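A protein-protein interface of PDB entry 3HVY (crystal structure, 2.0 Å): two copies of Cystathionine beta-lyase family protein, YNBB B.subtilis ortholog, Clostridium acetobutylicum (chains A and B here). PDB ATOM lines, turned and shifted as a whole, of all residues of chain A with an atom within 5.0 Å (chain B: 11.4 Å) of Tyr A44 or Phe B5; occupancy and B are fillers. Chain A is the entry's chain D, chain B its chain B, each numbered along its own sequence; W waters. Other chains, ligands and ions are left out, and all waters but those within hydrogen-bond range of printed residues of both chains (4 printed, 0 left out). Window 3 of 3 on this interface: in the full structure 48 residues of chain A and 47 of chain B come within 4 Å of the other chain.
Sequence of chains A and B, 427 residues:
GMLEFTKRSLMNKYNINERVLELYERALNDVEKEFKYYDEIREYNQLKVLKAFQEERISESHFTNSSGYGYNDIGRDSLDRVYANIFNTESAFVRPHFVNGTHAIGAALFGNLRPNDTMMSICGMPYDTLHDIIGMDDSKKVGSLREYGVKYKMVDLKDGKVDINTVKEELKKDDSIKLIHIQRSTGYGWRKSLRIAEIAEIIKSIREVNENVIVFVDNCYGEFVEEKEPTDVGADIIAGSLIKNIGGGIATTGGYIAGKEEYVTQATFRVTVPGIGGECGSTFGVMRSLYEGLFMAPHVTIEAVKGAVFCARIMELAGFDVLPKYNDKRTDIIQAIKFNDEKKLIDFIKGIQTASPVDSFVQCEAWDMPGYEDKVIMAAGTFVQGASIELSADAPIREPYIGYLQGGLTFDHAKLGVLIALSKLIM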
ATOM      1  N   GLU A  40       1.474  29.685 -28.336  1.00  0.00           N
ATOM      2  CA  GLU A  40       1.592  28.618 -27.311  1.00  0.00           C
ATOM      3  C   GLU A  40       1.405  27.241 -27.915  1.00  0.00           C
ATOM      4  O   GLU A  40       2.165  26.314 -27.640  1.00  0.00           O
ATOM      5  CB  GLU A  40       0.557  28.829 -26.227  1.00  0.00           C
ATOM      6  CG  GLU A  40       0.825  30.110 -25.421  1.00  0.00           C
ATOM      7  CD  GLU A  40      -0.316  30.432 -24.464  1.00  0.00           C
ATOM      8  OE1 GLU A  40      -1.241  29.602 -24.347  1.00  0.00           O
ATOM      9  OE2 GLU A  40      -0.288  31.520 -23.861  1.00  0.00           O
ATOM     10  N   ILE A  41       0.382  27.133 -28.761  1.00  0.00           N
ATOM     11  CA  ILE A  41       0.142  25.917 -29.501  1.00  0.00           C
ATOM     12  C   ILE A  41       1.283  25.635 -30.489  1.00  0.00           C
ATOM     13  O   ILE A  41       1.733  24.497 -30.604  1.00  0.00           O
ATOM     14  CB  ILE A  41      -1.219  26.001 -30.238  1.00  0.00           C
ATOM     15  CG1 ILE A  41      -2.378  25.927 -29.230  1.00  0.00           C
ATOM     16  CG2 ILE A  41      -1.362  24.865 -31.248  1.00  0.00           C
ATOM     17  CD1 ILE A  41      -3.736  26.050 -29.878  1.00  0.00           C
ATOM     18  N   ARG A  42       1.773  26.659 -31.191  1.00  0.00           N
ATOM     19  CA  ARG A  42       2.828  26.478 -32.160  1.00  0.00           C
ATOM     20  C   ARG A  42       4.082  25.933 -31.513  1.00  0.00           C
ATOM     21  O   ARG A  42       4.774  25.100 -32.081  1.00  0.00           O
ATOM     22  CB  ARG A  42       3.170  27.845 -32.754  1.00  0.00           C
ATOM     23  CG  ARG A  42       4.148  27.799 -33.819  1.00  0.00           C
ATOM     24  CD  ARG A  42       4.391  29.191 -34.440  1.00  0.00           C
ATOM     25  NE  ARG A  42       4.957  30.059 -33.419  1.00  0.00           N
ATOM     26  CZ  ARG A  42       5.102  31.374 -33.511  1.00  0.00           C
ATOM     27  NH1 ARG A  42       4.713  32.014 -34.571  1.00  0.00           N
ATOM     28  NH2 ARG A  42       5.649  32.042 -32.508  1.00  0.00           N
ATOM     29  N   GLU A  43       4.402  26.456 -30.334  1.00  0.00           N
ATOM     30  CA  GLU A  43       5.592  26.058 -29.612  1.00  0.00           C
ATOM     31  C   GLU A  43       5.535  24.552 -29.241  1.00  0.00           C
ATOM     32  O   GLU A  43       6.514  23.792 -29.374  1.00  0.00           O
ATOM     33  CB  GLU A  43       5.655  26.917 -28.369  1.00  0.00           C
ATOM     34  CG  GLU A  43       6.805  26.615 -27.461  1.00  0.00           C
ATOM     35  CD  GLU A  43       6.797  27.493 -26.216  1.00  0.00           C
ATOM     36  OE1 GLU A  43       5.870  27.350 -25.360  1.00  0.00           O
ATOM     37  OE2 GLU A  43       7.768  28.271 -26.076  1.00  0.00           O
ATOM     38  N   TYR A  44       4.370  24.145 -28.751  1.00  0.00           N
ATOM     39  CA  TYR A  44       4.126  22.764 -28.438  1.00  0.00           C
ATOM     40  C   TYR A  44       4.326  21.874 -29.690  1.00  0.00           C
ATOM     41  O   TYR A  44       5.039  20.879 -29.671  1.00  0.00           O
ATOM     42  CB  TYR A  44       2.697  22.613 -27.927  1.00  0.00           C
ATOM     43  CG  TYR A  44       2.414  21.172 -27.602  1.00  0.00           C
ATOM     44  CD1 TYR A  44       2.971  20.600 -26.479  1.00  0.00           C
ATOM     45  CD2 TYR A  44       1.620  20.381 -28.427  1.00  0.00           C
ATOM     46  CE1 TYR A  44       2.750  19.290 -26.165  1.00  0.00           C
ATOM     47  CE2 TYR A  44       1.388  19.054 -28.118  1.00  0.00           C
ATOM     48  CZ  TYR A  44       1.967  18.519 -26.976  1.00  0.00           C
ATOM     49  OH  TYR A  44       1.796  17.216 -26.591  1.00  0.00           O
ATOM     50  N   ASN A  45       3.656  22.241 -30.771  1.00  0.00           N
ATOM     51  CA  ASN A  45       3.729  21.477 -31.995  1.00  0.00           C
ATOM     52  C   ASN A  45       5.118  21.482 -32.615  1.00  0.00           C
ATOM     53  O   ASN A  45       5.545  20.477 -33.142  1.00  0.00           O
ATOM     54  CB  ASN A  45       2.663  21.955 -32.970  1.00  0.00           C
ATOM     55  CG  ASN A  45       1.287  21.505 -32.571  1.00  0.00           C
ATOM     56  OD1 ASN A  45       1.153  20.505 -31.867  1.00  0.00           O
ATOM     57  ND2 ASN A  45       0.238  22.182 -33.076  1.00  0.00           N
ATOM     58  N   GLN A  46       5.844  22.580 -32.513  1.00  0.00           N
ATOM     59  CA  GLN A  46       7.189  22.566 -33.018  1.00  0.00           C
ATOM     60  C   GLN A  46       8.029  21.530 -32.262  1.00  0.00           C
ATOM     61  O   GLN A  46       8.856  20.822 -32.847  1.00  0.00           O
ATOM     62  CB  GLN A  46       7.841  23.947 -32.910  1.00  0.00           C
ATOM     63  CG  GLN A  46       9.277  23.953 -33.424  1.00  0.00           C
ATOM     64  CD  GLN A  46       9.331  24.032 -34.907  1.00  0.00           C
ATOM     65  OE1 GLN A  46       9.201  25.112 -35.470  1.00  0.00           O
ATOM     66  NE2 GLN A  46       9.519  22.881 -35.570  1.00  0.00           N
ATOM     67  N   LEU A  47       7.859  21.505 -30.950  1.00  0.00           N
ATOM     68  CA  LEU A  47       8.535  20.558 -30.090  1.00  0.00           C
ATOM     69  C   LEU A  47       8.107  19.124 -30.369  1.00  0.00           C
ATOM     70  O   LEU A  47       8.914  18.229 -30.450  1.00  0.00           O
ATOM     71  CB  LEU A  47       8.249  20.903 -28.629  1.00  0.00           C
ATOM     72  CG  LEU A  47       8.857  19.959 -27.577  1.00  0.00           C
ATOM     73  CD1 LEU A  47      10.424  19.895 -27.669  1.00  0.00           C
ATOM     74  CD2 LEU A  47       8.409  20.413 -26.186  1.00  0.00           C
ATOM     75  N   LYS A  48       6.817  18.893 -30.549  1.00  0.00           N
ATOM     76  CA  LYS A  48       6.346  17.541 -30.906  1.00  0.00           C
ATOM     77  C   LYS A  48       7.070  17.004 -32.175  1.00  0.00           C
ATOM     78  O   LYS A  48       7.419  15.811 -32.285  1.00  0.00           O
ATOM     79  CB  LYS A  48       4.828  17.662 -31.127  1.00  0.00           C
ATOM     80  CG  LYS A  48       4.130  16.529 -31.770  1.00  0.00           C
ATOM     81  CD  LYS A  48       2.589  16.563 -31.502  1.00  0.00           C
ATOM     82  CE  LYS A  48       1.810  17.657 -32.182  1.00  0.00           C
ATOM     83  NZ  LYS A  48       0.259  17.463 -32.104  1.00  0.00           N
ATOM     84  N   GLU A 227      -3.237  21.511 -30.649  1.00  0.00           N
ATOM     85  CA  GLU A 227      -2.133  20.741 -30.055  1.00  0.00           C
ATOM     86  C   GLU A 227      -2.340  19.240 -30.187  1.00  0.00           C
ATOM     87  O   GLU A 227      -1.419  18.459 -29.944  1.00  0.00           O
ATOM     88  CB  GLU A 227      -1.901  21.190 -28.593  1.00  0.00           C
ATOM     89  CG  GLU A 227      -2.900  20.803 -27.561  1.00  0.00           C
ATOM     90  CD  GLU A 227      -4.346  21.334 -27.771  1.00  0.00           C
ATOM     91  OE1 GLU A 227      -4.630  22.359 -28.504  1.00  0.00           O
ATOM     92  OE2 GLU A 227      -5.217  20.674 -27.157  1.00  0.00           O
ATOM     93  N   GLY B   1       0.781  31.427 -21.122  1.00  0.00           N
ATOM     94  CA  GLY B   1       2.187  31.274 -21.608  1.00  0.00           C
ATOM     95  C   GLY B   1       2.387  29.829 -22.022  1.00  0.00           C
ATOM     96  O   GLY B   1       1.424  29.145 -22.419  1.00  0.00           O
ATOM     97  N   MET B   2       3.622  29.353 -21.888  1.00  0.00           N
ATOM     98  CA  MET B   2       3.993  27.992 -22.282  1.00  0.00           C
ATOM     99  C   MET B   2       3.018  26.966 -21.730  1.00  0.00           C
ATOM    100  O   MET B   2       2.737  26.958 -20.539  1.00  0.00           O
ATOM    101  CB  MET B   2       5.404  27.686 -21.783  1.00  0.00           C
ATOM    102  CG  MET B   2       5.866  26.254 -22.022  1.00  0.00           C
ATOM    103  SD  MET B   2       7.742  25.916 -21.437  1.00  0.00           S
ATOM    104  CE  MET B   2       8.659  26.861 -22.777  1.00  0.00           C
ATOM    105  N   LEU B   3       2.506  26.088 -22.584  1.00  0.00           N
ATOM    106  CA  LEU B   3       1.555  25.095 -22.145  1.00  0.00           C
ATOM    107  C   LEU B   3       2.235  24.125 -21.145  1.00  0.00           C
ATOM    108  O   LEU B   3       3.454  23.904 -21.183  1.00  0.00           O
ATOM    109  CB  LEU B   3       0.976  24.345 -23.354  1.00  0.00           C
ATOM    110  CG  LEU B   3       0.284  25.163 -24.494  1.00  0.00           C
ATOM    111  CD1 LEU B   3      -0.339  24.210 -25.550  1.00  0.00           C
ATOM    112  CD2 LEU B   3      -0.780  26.107 -23.927  1.00  0.00           C
ATOM    113  N   GLU B   4       1.444  23.537 -20.246  1.00  0.00           N
ATOM    114  CA  GLU B   4       2.007  22.665 -19.245  1.00  0.00           C
ATOM    115  C   GLU B   4       2.663  21.459 -19.890  1.00  0.00           C
ATOM    116  O   GLU B   4       3.738  21.010 -19.456  1.00  0.00           O
ATOM    117  CB  GLU B   4       0.931  22.216 -18.242  1.00  0.00           C
ATOM    118  CG  GLU B   4       1.534  21.604 -16.957  1.00  0.00           C
ATOM    119  CD  GLU B   4       2.465  22.594 -16.225  1.00  0.00           C
ATOM    120  OE1 GLU B   4       2.268  23.838 -16.392  1.00  0.00           O
ATOM    121  OE2 GLU B   4       3.392  22.120 -15.501  1.00  0.00           O
ATOM    122  N   PHE B   5       2.033  20.935 -20.935  1.00  0.00           N
ATOM    123  CA  PHE B   5       2.557  19.784 -21.619  1.00  0.00           C
ATOM    124  C   PHE B   5       3.881  20.122 -22.340  1.00  0.00           C
ATOM    125  O   PHE B   5       4.772  19.264 -22.484  1.00  0.00           O
ATOM    126  CB  PHE B   5       1.482  19.240 -22.579  1.00  0.00           C
ATOM    127  N   THR B   6       4.036  21.375 -22.783  1.00  0.00           N
ATOM    128  CA  THR B   6       5.343  21.802 -23.374  1.00  0.00           C
ATOM    129  C   THR B   6       6.415  21.770 -22.267  1.00  0.00           C
ATOM    130  O   THR B   6       7.497  21.201 -22.423  1.00  0.00           O
ATOM    131  CB  THR B   6       5.277  23.213 -23.897  1.00  0.00           C
ATOM    132  OG1 THR B   6       4.220  23.333 -24.862  1.00  0.00           O
ATOM    133  CG2 THR B   6       6.627  23.659 -24.539  1.00  0.00           C
ATOM    134  N   LYS B   7       6.092  22.385 -21.133  1.00  0.00           N
ATOM    135  CA  LYS B   7       7.003  22.433 -19.971  1.00  0.00           C
ATOM    136  C   LYS B   7       7.446  21.019 -19.579  1.00  0.00           C
ATOM    137  O   LYS B   7       8.639  20.710 -19.507  1.00  0.00           O
ATOM    138  CB  LYS B   7       6.284  23.163 -18.828  1.00  0.00           C
ATOM    139  CG  LYS B   7       7.116  23.496 -17.609  1.00  0.00           C
ATOM    140  CD  LYS B   7       6.240  24.101 -16.486  1.00  0.00           C
ATOM    141  N   ARG B   8       6.487  20.129 -19.423  1.00  0.00           N
ATOM    142  CA  ARG B   8       6.785  18.765 -19.036  1.00  0.00           C
ATOM    143  C   ARG B   8       7.630  18.042 -20.050  1.00  0.00           C
ATOM    144  O   ARG B   8       8.536  17.314 -19.704  1.00  0.00           O
ATOM    145  CB  ARG B   8       5.480  17.970 -18.805  1.00  0.00           C
ATOM    146  CG  ARG B   8       4.715  18.392 -17.528  1.00  0.00           C
ATOM    147  CD  ARG B   8       3.423  17.586 -17.311  1.00  0.00           C
ATOM    148  NE  ARG B   8       2.444  18.301 -16.481  1.00  0.00           N
ATOM    149  N   SER B   9       7.317  18.221 -21.314  1.00  0.00           N
ATOM    150  CA  SER B   9       8.049  17.540 -22.362  1.00  0.00           C
ATOM    151  C   SER B   9       9.496  18.018 -22.406  1.00  0.00           C
ATOM    152  O   SER B   9      10.424  17.219 -22.537  1.00  0.00           O
ATOM    153  CB  SER B   9       7.350  17.830 -23.692  1.00  0.00           C
ATOM    154  OG  SER B   9       7.999  17.198 -24.761  1.00  0.00           O
ATOM    155  N   LEU B  10       9.680  19.331 -22.302  1.00  0.00           N
ATOM    156  CA  LEU B  10      11.014  19.921 -22.246  1.00  0.00           C
ATOM    157  C   LEU B  10      11.830  19.395 -21.087  1.00  0.00           C
ATOM    158  O   LEU B  10      12.981  19.013 -21.245  1.00  0.00           O
ATOM    159  CB  LEU B  10      10.901  21.422 -22.111  1.00  0.00           C
ATOM    160  CG  LEU B  10      10.503  22.183 -23.353  1.00  0.00           C
ATOM    161  CD1 LEU B  10      10.431  23.628 -22.930  1.00  0.00           C
ATOM    162  CD2 LEU B  10      11.550  21.978 -24.510  1.00  0.00           C
ATOM    163  N   MET B  11      11.215  19.344 -19.914  1.00  0.00           N
ATOM    164  CA  MET B  11      11.900  18.864 -18.724  1.00  0.00           C
ATOM    165  C   MET B  11      12.243  17.391 -18.835  1.00  0.00           C
ATOM    166  O   MET B  11      13.383  17.011 -18.624  1.00  0.00           O
ATOM    167  CB  MET B  11      11.048  19.143 -17.469  1.00  0.00           C
ATOM    168  CG  MET B  11      10.911  20.630 -17.194  1.00  0.00           C
ATOM    169  SD  MET B  11       9.946  21.003 -15.506  1.00  0.00           S
ATOM    170  CE  MET B  11      11.117  22.518 -14.981  1.00  0.00           C
ATOM    171  N   ASN B  12      11.279  16.583 -19.238  1.00  0.00           N
ATOM    172  CA  ASN B  12      11.481  15.155 -19.332  1.00  0.00           C
ATOM    173  C   ASN B  12      12.409  14.717 -20.454  1.00  0.00           C
ATOM    174  O   ASN B  12      13.209  13.807 -20.263  1.00  0.00           O
ATOM    175  CB  ASN B  12      10.132  14.427 -19.451  1.00  0.00           C
ATOM    176  CG  ASN B  12       9.248  14.607 -18.199  1.00  0.00           C
ATOM    177  OD1 ASN B  12       9.713  15.064 -17.136  1.00  0.00           O
ATOM    178  ND2 ASN B  12       7.967  14.266 -18.333  1.00  0.00           N
ATOM    179  N   LYS B  13      12.326  15.362 -21.607  1.00  0.00           N
ATOM    180  CA  LYS B  13      13.140  14.966 -22.724  1.00  0.00           C
ATOM    181  C   LYS B  13      14.522  15.562 -22.667  1.00  0.00           C
ATOM    182  O   LYS B  13      15.482  14.882 -22.993  1.00  0.00           O
ATOM    183  CB  LYS B  13      12.445  15.397 -24.019  1.00  0.00           C
ATOM    184  CG  LYS B  13      13.206  15.195 -25.348  1.00  0.00           C
ATOM    185  CD  LYS B  13      13.234  13.735 -25.789  1.00  0.00           C
ATOM    186  CE  LYS B  13      13.631  13.616 -27.258  1.00  0.00           C
ATOM    187  NZ  LYS B  13      13.911  12.203 -27.599  1.00  0.00           N
ATOM    188  N   TYR B  14      14.635  16.842 -22.307  1.00  0.00           N
ATOM    189  CA  TYR B  14      15.917  17.530 -22.415  1.00  0.00           C
ATOM    190  C   TYR B  14      16.504  17.974 -21.069  1.00  0.00           C
ATOM    191  O   TYR B  14      17.549  18.615 -21.044  1.00  0.00           O
ATOM    192  CB  TYR B  14      15.799  18.707 -23.362  1.00  0.00           C
ATOM    193  CG  TYR B  14      15.297  18.338 -24.777  1.00  0.00           C
ATOM    194  CD1 TYR B  14      16.114  17.655 -25.681  1.00  0.00           C
ATOM    195  CD2 TYR B  14      14.031  18.701 -25.202  1.00  0.00           C
ATOM    196  CE1 TYR B  14      15.668  17.341 -26.965  1.00  0.00           C
ATOM    197  CE2 TYR B  14      13.580  18.376 -26.455  1.00  0.00           C
ATOM    198  CZ  TYR B  14      14.411  17.698 -27.344  1.00  0.00           C
ATOM    199  OH  TYR B  14      13.954  17.371 -28.606  1.00  0.00           O
ATOM    200  N   ILE B  16      15.455  20.239 -19.157  1.00  0.00           N
ATOM    201  CA  ILE B  16      15.404  21.678 -18.996  1.00  0.00           C
ATOM    202  C   ILE B  16      14.938  21.909 -17.537  1.00  0.00           C
ATOM    203  O   ILE B  16      14.101  21.162 -17.011  1.00  0.00           O
ATOM    204  CB  ILE B  16      14.566  22.308 -20.097  1.00  0.00           C
ATOM    205  CG1 ILE B  16      15.375  22.205 -21.414  1.00  0.00           C
ATOM    206  CG2 ILE B  16      14.239  23.762 -19.773  1.00  0.00           C
ATOM    207  CD1 ILE B  16      14.634  22.634 -22.617  1.00  0.00           C
ATOM    208  N   LEU B  21      13.828  27.891 -17.152  1.00  0.00           N
ATOM    209  CA  LEU B  21      12.451  28.267 -17.500  1.00  0.00           C
ATOM    210  C   LEU B  21      12.026  29.621 -16.909  1.00  0.00           C
ATOM    211  O   LEU B  21      11.268  30.339 -17.530  1.00  0.00           O
ATOM    212  CB  LEU B  21      11.478  27.173 -17.075  1.00  0.00           C
ATOM    213  CG  LEU B  21      11.435  25.908 -17.953  1.00  0.00           C
ATOM    214  CD1 LEU B  21      10.480  24.842 -17.362  1.00  0.00           C
ATOM    215  CD2 LEU B  21      11.049  26.230 -19.396  1.00  0.00           C
ATOM    216  N   TYR B  24      13.708  32.118 -19.111  1.00  0.00           N
ATOM    217  CA  TYR B  24      12.966  32.163 -20.368  1.00  0.00           C
ATOM    218  C   TYR B  24      11.805  33.165 -20.331  1.00  0.00           C
ATOM    219  O   TYR B  24      11.650  33.976 -21.273  1.00  0.00           O
ATOM    220  CB  TYR B  24      12.443  30.790 -20.703  1.00  0.00           C
ATOM    221  CG  TYR B  24      11.420  30.781 -21.808  1.00  0.00           C
ATOM    222  CD1 TYR B  24      11.724  31.288 -23.040  1.00  0.00           C
ATOM    223  CD2 TYR B  24      10.145  30.259 -21.606  1.00  0.00           C
ATOM    224  CE1 TYR B  24      10.808  31.277 -24.057  1.00  0.00           C
ATOM    225  CE2 TYR B  24       9.209  30.249 -22.621  1.00  0.00           C
ATOM    226  CZ  TYR B  24       9.558  30.742 -23.845  1.00  0.00           C
ATOM    227  OH  TYR B  24       8.640  30.741 -24.873  1.00  0.00           O
ATOM    228  N   THR B 410      12.710  28.677 -37.526  1.00  0.00           N
ATOM    229  CA  THR B 410      11.601  29.297 -36.788  1.00  0.00           C
ATOM    230  C   THR B 410      12.184  29.794 -35.459  1.00  0.00           C
ATOM    231  O   THR B 410      13.174  29.273 -35.007  1.00  0.00           O
ATOM    232  CB  THR B 410      10.494  28.312 -36.561  1.00  0.00           C
ATOM    233  OG1 THR B 410      10.900  27.355 -35.557  1.00  0.00           O
ATOM    234  CG2 THR B 410      10.072  27.636 -37.929  1.00  0.00           C
ATOM    235  N   PHE B 411      11.590  30.820 -34.856  1.00  0.00           N
ATOM    236  CA  PHE B 411      12.038  31.298 -33.563  1.00  0.00           C
ATOM    237  C   PHE B 411      11.836  30.219 -32.513  1.00  0.00           C
ATOM    238  O   PHE B 411      12.661  30.046 -31.615  1.00  0.00           O
ATOM    239  CB  PHE B 411      11.294  32.617 -33.174  1.00  0.00           C
ATOM    240  CG  PHE B 411      11.486  33.024 -31.752  1.00  0.00           C
ATOM    241  CD1 PHE B 411      12.730  33.421 -31.281  1.00  0.00           C
ATOM    242  CD2 PHE B 411      10.422  33.022 -30.873  1.00  0.00           C
ATOM    243  CE1 PHE B 411      12.903  33.775 -29.960  1.00  0.00           C
ATOM    244  CE2 PHE B 411      10.585  33.386 -29.568  1.00  0.00           C
ATOM    245  CZ  PHE B 411      11.827  33.760 -29.098  1.00  0.00           C
ATOM    246  N   ASP B 412      10.750  29.461 -32.620  1.00  0.00           N
ATOM    247  CA  ASP B 412      10.530  28.363 -31.663  1.00  0.00           C
ATOM    248  C   ASP B 412      11.707  27.394 -31.603  1.00  0.00           C
ATOM    249  O   ASP B 412      12.133  26.972 -30.522  1.00  0.00           O
ATOM    250  CB  ASP B 412       9.238  27.623 -32.014  1.00  0.00           C
ATOM    251  CG  ASP B 412       7.994  28.375 -31.600  1.00  0.00           C
ATOM    252  OD1 ASP B 412       7.963  28.935 -30.478  1.00  0.00           O
ATOM    253  OD2 ASP B 412       6.998  28.366 -32.373  1.00  0.00           O
ATOM    254  N   HIS B 413      12.275  27.050 -32.762  1.00  0.00           N
ATOM    255  CA  HIS B 413      13.411  26.148 -32.832  1.00  0.00           C
ATOM    256  C   HIS B 413      14.653  26.783 -32.216  1.00  0.00           C
ATOM    257  O   HIS B 413      15.265  26.210 -31.342  1.00  0.00           O
ATOM    258  CB  HIS B 413      13.698  25.650 -34.258  1.00  0.00           C
ATOM    259  CG  HIS B 413      14.820  24.638 -34.313  1.00  0.00           C
ATOM    260  ND1 HIS B 413      15.752  24.582 -35.334  1.00  0.00           N
ATOM    261  CD2 HIS B 413      15.142  23.644 -33.456  1.00  0.00           C
ATOM    262  CE1 HIS B 413      16.612  23.609 -35.085  1.00  0.00           C
ATOM    263  NE2 HIS B 413      16.254  23.011 -33.961  1.00  0.00           N
ATOM    264  N   LYS B 415      14.816  29.292 -30.038  1.00  0.00           N
ATOM    265  CA  LYS B 415      14.514  29.411 -28.587  1.00  0.00           C
ATOM    266  C   LYS B 415      14.721  28.086 -27.887  1.00  0.00           C
ATOM    267  O   LYS B 415      15.435  28.014 -26.874  1.00  0.00           O
ATOM    268  CB  LYS B 415      13.059  29.900 -28.408  1.00  0.00           C
ATOM    269  CG  LYS B 415      12.342  29.492 -27.152  1.00  0.00           C
ATOM    270  CD  LYS B 415      10.934  30.126 -27.056  1.00  0.00           C
ATOM    271  CE  LYS B 415      10.083  29.925 -28.225  1.00  0.00           C
ATOM    272  NZ  LYS B 415       8.644  30.045 -27.932  1.00  0.00           N
ATOM    273  N   LEU B 416      14.131  27.022 -28.426  1.00  0.00           N
ATOM    274  CA  LEU B 416      14.205  25.703 -27.779  1.00  0.00           C
ATOM    275  C   LEU B 416      15.648  25.249 -27.701  1.00  0.00           C
ATOM    276  O   LEU B 416      16.097  24.726 -26.717  1.00  0.00           O
ATOM    277  CB  LEU B 416      13.358  24.658 -28.514  1.00  0.00           C
ATOM    278  CG  LEU B 416      11.818  24.835 -28.499  1.00  0.00           C
ATOM    279  CD1 LEU B 416      11.043  23.904 -29.519  1.00  0.00           C
ATOM    280  CD2 LEU B 416      11.267  24.663 -27.105  1.00  0.00           C
ATOM    281  N   LEU B 419      17.454  27.050 -24.833  1.00  0.00           N
ATOM    282  CA  LEU B 419      17.066  26.500 -23.524  1.00  0.00           C
ATOM    283  C   LEU B 419      17.766  25.167 -23.233  1.00  0.00           C
ATOM    284  O   LEU B 419      18.209  24.929 -22.136  1.00  0.00           O
ATOM    285  CB  LEU B 419      15.562  26.273 -23.467  1.00  0.00           C
ATOM    286  CG  LEU B 419      14.710  27.548 -23.626  1.00  0.00           C
ATOM    287  CD1 LEU B 419      13.210  27.168 -23.491  1.00  0.00           C
ATOM    288  CD2 LEU B 419      15.104  28.668 -22.647  1.00  0.00           C
HETATM  289  O   HOH W   1       8.295  30.340 -34.253  1.00  0.00           O
HETATM  290  O   HOH W   2       7.498  27.397 -34.865  1.00  0.00           O
HETATM  291  O   HOH W   3       5.650  30.390 -30.060  1.00  0.00           O
HETATM  292  O   HOH W   4       3.595  26.002 -25.257  1.00  0.00           O
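Glu A43 touches just these residues of chain B: Met B2 (3.5 Å), Thr B6 (3.9 Å), Tyr B24 (2.9 Å), Asp B412 (3.7 Å) and Lys B415 (2.7 Å). Of chain B, only Phe B5 (3.8 Å) and Thr B6 (3.4 Å) come within 4 Å of Tyr A44. No residue of chain B comes within 4 Å of Asn A45. Leu A47 touches just these residues of chain B: Thr B6, Ser B9, Leu B10 and Tyr B14. No residue of chain B comes within 4 Å of Lys A48. No residue of chain B comes within 4 Å of Glu A227. Printed residues of chain A within 4 Å of Gly B1: Glu A40 (2.9 Å). Glu B4 touches none of the printed residues of chain A. Printed residues of chain A within 4 Å of Phe B5: Tyr A44. Printed residues of chain A within 4 Å of Thr B6: Glu A43 (3.9 Å), Tyr A44 (3.4 Å) and Leu A47 (3.95 Å). Printed residues of chain A within 4 Å of Tyr B14: Leu A47. The nearest residue of chain B that does not touch Tyr A44 is Leu B3 (4.2 Å). The nearest printed residue of chain A that does not touch Phe B5 is Leu A47 (5.3 Å). The nearest printed residue of chain A that does not touch Leu B10 is Glu A43 (6.2 Å).
Among the printed residues, pairs that only touch across the chains: Glu A40 with Leu B3, Glu A43 with Met B2, Glu A43 with Thr B6, Glu A43 with Asp B412, Tyr A44 with Phe B5, Tyr A44 with Thr B6, Gln A46 with Asp B412, Leu A47 with Thr B6, Leu A47 with Ser B9, Leu A47 with Leu B10 and Leu A47 with Tyr B14.
The side-chain hydroxyl of Thr B410 is in hydrogen-bond range of the side-chain amide oxygen of Gln A46 (2.8 Å). The side-chain amino group (NZ) of Lys B415 is in salt-bridge range of the side-chain carboxylate (OE2) of Glu A43. The side-chain hydroxyl (OH) of Tyr B24 lies within hydrogen-bond range of the side-chain carboxylate (OE2) of Glu A43. NE of Arg A42 lies within salt-bridge range of OD2 of Asp B412 (2.9 Å). N of Gly B1 lies within hydrogen-bond range of OE2 of Glu A40 (2.9 Å).
Water W4 lies within hydrogen-bond range of OE1 of Glu A43 (2.6 Å), OG1 of Thr B6 (2.8 Å), O of Glu A40 (2.8 Å) and N of Leu B3 (2.9 Å). Water W3 lies within hydrogen-bond range of OD1 of Asp B412 (2.8 Å) and NH2 of Arg A42 (3.0 Å). Water W1 lies within hydrogen-bond range of the side-chain carboxylate (OD2) of Asp B412 (3.0 Å), the backbone NH (N) of Phe B411 (3.4 Å) and the guanidinium group (NE) of Arg A42 (3.5 Å).
Hydrophobic or aromatic side chains of chain B that line the printed part of chain A: Met B2, Leu B3, Phe B5, Leu B10, Tyr B14 and Tyr B24. Of the 10 printed residues of chain A, 6 touch a printed residue of chain B. Hydrophobic or aromatic side chains of chain A that line the printed part of chain B: Tyr A44 and Leu A47. Along chain A the printed residues that touch a printed residue of chain B span positions 40 to 47. Among the printed residues, 16 pairs touch across the chains. Among the printed residues, Asp or Glu carboxylates within 4 Å of a Lys or Arg side-chain nitrogen of the other chain: Arg A42 with Asp B412 (2.9 Å) and Glu A43 with Lys B415 (2.7 Å).
The side-chain carboxylate (OD1) of Asp B412 is in salt-bridge range of the side-chain amino group (NZ) of Lys B415 (2.9 Å). O of Leu B10 is in hydrogen-bond range of N of Ile B16, at 3.5 Å. The side-chain hydroxyl of Thr B410 sits at hydrogen-bond distance from the backbone NH of His B413 (3.1 Å). The side-chain amino group of Lys B415 sits at hydrogen-bond distance from the side-chain hydroxyl of Tyr B24 (3.1 Å).
No position is printed for both chains.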
